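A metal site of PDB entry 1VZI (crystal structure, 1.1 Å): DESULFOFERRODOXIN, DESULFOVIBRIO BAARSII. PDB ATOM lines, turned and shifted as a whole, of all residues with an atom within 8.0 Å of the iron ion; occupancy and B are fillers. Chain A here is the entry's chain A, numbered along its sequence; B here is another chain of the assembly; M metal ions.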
ATOM      1  N   LYS A   9      25.442  -4.746  -8.511  1.00  0.00           N
ATOM      2  CA  LYS A   9      24.658  -5.327  -9.597  1.00  0.00           C
ATOM      3  C   LYS A   9      24.460  -4.361 -10.734  1.00  0.00           C
ATOM      4  O   LYS A   9      24.121  -3.204 -10.526  1.00  0.00           O
ATOM      5  CB  LYS A   9      23.253  -5.739  -9.044  1.00  0.00           C
ATOM      6  CG  LYS A   9      22.318  -6.168 -10.165  1.00  0.00           C
ATOM      7  CD  LYS A   9      20.949  -6.628  -9.663  1.00  0.00           C
ATOM      8  CE  LYS A   9      20.171  -7.201 -10.891  1.00  0.00           C
ATOM      9  NZ  LYS A   9      18.786  -7.592 -10.481  1.00  0.00           N
ATOM     10  N   CYS A  10      24.601  -4.891 -11.970  1.00  0.00           N
ATOM     11  CA  CYS A  10      24.135  -4.137 -13.126  1.00  0.00           C
ATOM     12  C   CYS A  10      22.652  -4.417 -13.376  1.00  0.00           C
ATOM     13  O   CYS A  10      22.258  -5.577 -13.651  1.00  0.00           O
ATOM     14  CB  CYS A  10      24.916  -4.558 -14.362  1.00  0.00           C
ATOM     15  SG  CYS A  10      24.326  -3.621 -15.824  1.00  0.00           S
ATOM     16  N   GLU A  11      21.823  -3.353 -13.275  1.00  0.00           N
ATOM     17  CA  GLU A  11      20.400  -3.599 -13.444  1.00  0.00           C
ATOM     18  C   GLU A  11      20.021  -3.713 -14.903  1.00  0.00           C
ATOM     19  O   GLU A  11      18.842  -3.989 -15.163  1.00  0.00           O
ATOM     20  CB  GLU A  11      19.616  -2.480 -12.723  1.00  0.00           C
ATOM     21  CG  GLU A  11      19.899  -2.540 -11.209  1.00  0.00           C
ATOM     22  CD  GLU A  11      18.926  -1.570 -10.568  1.00  0.00           C
ATOM     23  OE1 GLU A  11      19.205  -0.356 -10.543  1.00  0.00           O
ATOM     24  OE2 GLU A  11      17.905  -2.135 -10.134  1.00  0.00           O
ATOM     25  N   VAL A  12      20.941  -3.536 -15.818  1.00  0.00           N
ATOM     26  CA  VAL A  12      20.588  -3.719 -17.242  1.00  0.00           C
ATOM     27  C   VAL A  12      20.798  -5.183 -17.618  1.00  0.00           C
ATOM     28  O   VAL A  12      19.857  -5.859 -18.016  1.00  0.00           O
ATOM     29  CB  VAL A  12      21.449  -2.793 -18.117  1.00  0.00           C
ATOM     30  CG1 VAL A  12      21.181  -3.073 -19.616  1.00  0.00           C
ATOM     31  CG2 VAL A  12      21.178  -1.302 -17.809  1.00  0.00           C
ATOM     32  N   CYS A  13      22.047  -5.656 -17.456  1.00  0.00           N
ATOM     33  CA  CYS A  13      22.360  -6.965 -18.001  1.00  0.00           C
ATOM     34  C   CYS A  13      22.440  -8.017 -16.907  1.00  0.00           C
ATOM     35  O   CYS A  13      22.589  -9.203 -17.232  1.00  0.00           O
ATOM     36  CB  CYS A  13      23.678  -6.949 -18.781  1.00  0.00           C
ATOM     37  SG  CYS A  13      25.185  -6.885 -17.751  1.00  0.00           S
ATOM     38  N   GLY A  14      22.407  -7.642 -15.633  1.00  0.00           N
ATOM     39  CA  GLY A  14      22.390  -8.629 -14.556  1.00  0.00           C
ATOM     40  C   GLY A  14      23.764  -9.104 -14.067  1.00  0.00           C
ATOM     41  O   GLY A  14      23.745  -9.951 -13.161  1.00  0.00           O
ATOM     42  N   ASN A  15      24.889  -8.585 -14.571  1.00  0.00           N
ATOM     43  CA  ASN A  15      26.150  -8.884 -13.922  1.00  0.00           C
ATOM     44  C   ASN A  15      26.052  -8.541 -12.439  1.00  0.00           C
ATOM     45  O   ASN A  15      25.513  -7.493 -12.092  1.00  0.00           O
ATOM     46  CB  ASN A  15      27.262  -8.006 -14.520  1.00  0.00           C
ATOM     47  CG  ASN A  15      27.861  -8.535 -15.802  1.00  0.00           C
ATOM     48  OD1 ASN A  15      27.802  -9.740 -16.073  1.00  0.00           O
ATOM     49  ND2 ASN A  15      28.436  -7.622 -16.583  1.00  0.00           N
ATOM     50  N   ILE A  16      26.606  -9.402 -11.584  1.00  0.00           N
ATOM     51  CA  ILE A  16      26.706  -9.101 -10.155  1.00  0.00           C
ATOM     52  C   ILE A  16      28.149  -9.463  -9.734  1.00  0.00           C
ATOM     53  O   ILE A  16      28.603 -10.555 -10.105  1.00  0.00           O
ATOM     54  CB  ILE A  16      25.688  -9.864  -9.294  1.00  0.00           C
ATOM     55  CG1 ILE A  16      24.258  -9.511  -9.757  1.00  0.00           C
ATOM     56  CG2 ILE A  16      25.895  -9.527  -7.820  1.00  0.00           C
ATOM     57  CD1 ILE A  16      23.161 -10.359  -9.118  1.00  0.00           C
ATOM     58  N   VAL A  28      30.971   0.470 -13.147  1.00  0.00           N
ATOM     59  CA  VAL A  28      30.040   0.792 -14.225  1.00  0.00           C
ATOM     60  C   VAL A  28      29.820  -0.434 -15.111  1.00  0.00           C
ATOM     61  O   VAL A  28      30.729  -1.224 -15.359  1.00  0.00           O
ATOM     62  CB  VAL A  28      30.542   1.992 -15.061  1.00  0.00           C
ATOM     63  CG1 VAL A  28      29.721   2.159 -16.328  1.00  0.00           C
ATOM     64  CG2 VAL A  28      30.432   3.263 -14.201  1.00  0.00           C
ATOM     65  N   CYS A  29      28.590  -0.632 -15.602  1.00  0.00           N
ATOM     66  CA  CYS A  29      28.270  -1.703 -16.519  1.00  0.00           C
ATOM     67  C   CYS A  29      27.082  -1.221 -17.364  1.00  0.00           C
ATOM     68  O   CYS A  29      26.213  -0.507 -16.855  1.00  0.00           O
ATOM     69  CB  CYS A  29      27.931  -2.996 -15.754  1.00  0.00           C
ATOM     70  SG  CYS A  29      27.837  -4.427 -16.857  1.00  0.00           S
ATOM     71  N   CYS A  30      27.098  -1.526 -18.638  1.00  0.00           N
ATOM     72  CA  CYS A  30      25.980  -1.111 -19.543  1.00  0.00           C
ATOM     73  C   CYS A  30      25.767   0.391 -19.465  1.00  0.00           C
ATOM     74  O   CYS A  30      24.638   0.890 -19.478  1.00  0.00           O
ATOM     75  CB  CYS A  30      24.685  -1.850 -19.213  1.00  0.00           C
ATOM     76  SG  CYS A  30      24.864  -3.645 -19.507  1.00  0.00           S
ATOM     77  N   ASN A  31      26.867   1.122 -19.353  1.00  0.00           N
ATOM     78  CA  ASN A  31      26.823   2.592 -19.340  1.00  0.00           C
ATOM     79  C   ASN A  31      26.125   3.266 -18.181  1.00  0.00           C
ATOM     80  O   ASN A  31      25.689   4.437 -18.315  1.00  0.00           O
ATOM     81  CB  ASN A  31      26.094   3.033 -20.635  1.00  0.00           C
ATOM     82  CG  ASN A  31      27.171   3.207 -21.679  1.00  0.00           C
ATOM     83  OD1 ASN A  31      28.123   2.399 -21.781  1.00  0.00           O
ATOM     84  ND2 ASN A  31      26.947   4.294 -22.405  1.00  0.00           N
ATOM     85  N   GLN A  32      26.007   2.516 -17.065  1.00  0.00           N
ATOM     86  CA  GLN A  32      25.475   3.188 -15.865  1.00  0.00           C
ATOM     87  C   GLN A  32      26.164   2.585 -14.652  1.00  0.00           C
ATOM     88  O   GLN A  32      26.696   1.478 -14.658  1.00  0.00           O
ATOM     89  CB  GLN A  32      23.980   3.061 -15.692  1.00  0.00           C
ATOM     90  CG  GLN A  32      23.439   1.645 -15.623  1.00  0.00           C
ATOM     91  CD  GLN A  32      21.932   1.506 -15.675  1.00  0.00           C
ATOM     92  OE1 GLN A  32      21.233   0.797 -14.917  1.00  0.00           O
ATOM     93  NE2 GLN A  32      21.324   2.264 -16.583  1.00  0.00           N
ATOM     94  N   MET A  34      26.850   0.710 -11.432  1.00  0.00           N
ATOM     95  CA  MET A  34      26.301  -0.523 -10.826  1.00  0.00           C
ATOM     96  C   MET A  34      25.727  -0.162  -9.474  1.00  0.00           C
ATOM     97  O   MET A  34      26.239   0.775  -8.793  1.00  0.00           O
ATOM     98  CB  MET A  34      27.407  -1.593 -10.666  1.00  0.00           C
ATOM     99  CG  MET A  34      27.969  -2.035 -12.046  1.00  0.00           C
ATOM    100  SD  MET A  34      29.228  -3.358 -11.891  1.00  0.00           S
ATOM    101  CE  MET A  34      28.127  -4.779 -11.694  1.00  0.00           C
ATOM    102  N   PRO B   2      30.666 -11.346 -18.978  1.00  0.00           N
ATOM    103  CA  PRO B   2      31.498 -11.963 -17.878  1.00  0.00           C
ATOM    104  C   PRO B   2      30.867 -13.261 -17.388  1.00  0.00           C
ATOM    105  O   PRO B   2      29.683 -13.466 -17.570  1.00  0.00           O
ATOM    106  CB  PRO B   2      31.436 -10.869 -16.806  1.00  0.00           C
ATOM    107  CG  PRO B   2      31.461  -9.591 -17.610  1.00  0.00           C
ATOM    108  CD  PRO B   2      30.779  -9.889 -18.931  1.00  0.00           C
ATOM    109  N   GLY B  23      26.838 -12.172 -17.185  1.00  0.00           N
ATOM    110  CA  GLY B  23      25.926 -11.327 -17.999  1.00  0.00           C
ATOM    111  C   GLY B  23      26.725 -10.866 -19.214  1.00  0.00           C
ATOM    112  O   GLY B  23      27.938 -11.172 -19.320  1.00  0.00           O
ATOM    113  N   ILE B  24      26.034 -10.161 -20.117  1.00  0.00           N
ATOM    114  CA  ILE B  24      26.781  -9.823 -21.356  1.00  0.00           C
ATOM    115  C   ILE B  24      27.467  -8.470 -21.297  1.00  0.00           C
ATOM    116  O   ILE B  24      28.338  -8.224 -22.146  1.00  0.00           O
ATOM    117  CB  ILE B  24      25.819  -9.933 -22.571  1.00  0.00           C
ATOM    118  CG1 ILE B  24      24.709  -8.912 -22.455  1.00  0.00           C
ATOM    119  CG2 ILE B  24      25.258 -11.351 -22.736  1.00  0.00           C
ATOM    120  CD1 ILE B  24      23.736  -9.093 -23.668  1.00  0.00           C
ATOM    121  N   GLY B  25      27.181  -7.567 -20.325  1.00  0.00           N
ATOM    122  CA  GLY B  25      27.835  -6.256 -20.363  1.00  0.00           C
ATOM    123  C   GLY B  25      29.306  -6.297 -19.947  1.00  0.00           C
ATOM    124  O   GLY B  25      29.778  -7.132 -19.138  1.00  0.00           O
ATOM    125  N   GLU B  26      30.063  -5.354 -20.498  1.00  0.00           N
ATOM    126  CA  GLU B  26      31.467  -5.268 -20.149  1.00  0.00           C
ATOM    127  C   GLU B  26      31.621  -4.464 -18.868  1.00  0.00           C
ATOM    128  O   GLU B  26      31.100  -3.346 -18.770  1.00  0.00           O
ATOM    129  CB  GLU B  26      32.307  -4.675 -21.283  1.00  0.00           C
ATOM    130  CG  GLU B  26      32.338  -5.591 -22.510  1.00  0.00           C
ATOM    131  CD  GLU B  26      32.808  -5.005 -23.814  1.00  0.00           C
ATOM    132  OE1 GLU B  26      32.806  -3.765 -23.986  1.00  0.00           O
ATOM    133  OE2 GLU B  26      33.184  -5.803 -24.728  1.00  0.00           O
ATOM    134  N   LEU B  27      32.378  -4.965 -17.885  1.00  0.00           N
ATOM    135  CA  LEU B  27      32.586  -4.199 -16.663  1.00  0.00           C
ATOM    136  C   LEU B  27      33.593  -3.073 -16.889  1.00  0.00           C
ATOM    137  O   LEU B  27      34.653  -3.288 -17.532  1.00  0.00           O
ATOM    138  CB  LEU B  27      33.169  -5.118 -15.583  1.00  0.00           C
ATOM    139  CG  LEU B  27      32.229  -6.260 -15.191  1.00  0.00           C
ATOM    140  CD1 LEU B  27      32.980  -7.283 -14.353  1.00  0.00           C
ATOM    141  CD2 LEU B  27      30.999  -5.742 -14.434  1.00  0.00           C
HETATM  142 FE    FE M   1      25.645  -4.580 -17.524  1.00  0.00          FE
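The side-chain sulfur of Cys 10 lies close to the backbone NH of Val 12 (3.4 Å). The side-chain sulfur (SG) of Cys 13 lies close to the backbone NH (N) of Gly 25 of chain B, 3.3 Å away. The backbone carbonyl oxygen of Gly 25 of chain B lies within hydrogen-bond range of the side-chain amide nitrogen of Asn 15 (2.9 Å). The backbone NH (N) of Cys 10 is in hydrogen-bond range of the backbone carbonyl oxygen (O) of Asn 15. The side-chain sulfur (SG) of Cys 13 sits close to the side-chain amide nitrogen (ND2) of Asn 15 (3.5 Å). SG of Cys 29 sits close to ND2 of Asn 15 (3.3 Å).
CA of Gly 25 of chain B touches the iron ion (3.96 Å). Of the 20 residues printed, 5 come within 4 Å of the iron ion.
SG of Cys 29 is bound to the iron ion. SG of Cys 30 binds the iron ion, 2.3 Å away. SG of Cys 10 binds the iron ion. SG of Cys 13 is bound to the iron ion (2.4 Å). The iron ion has four donor atoms within binding distance.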
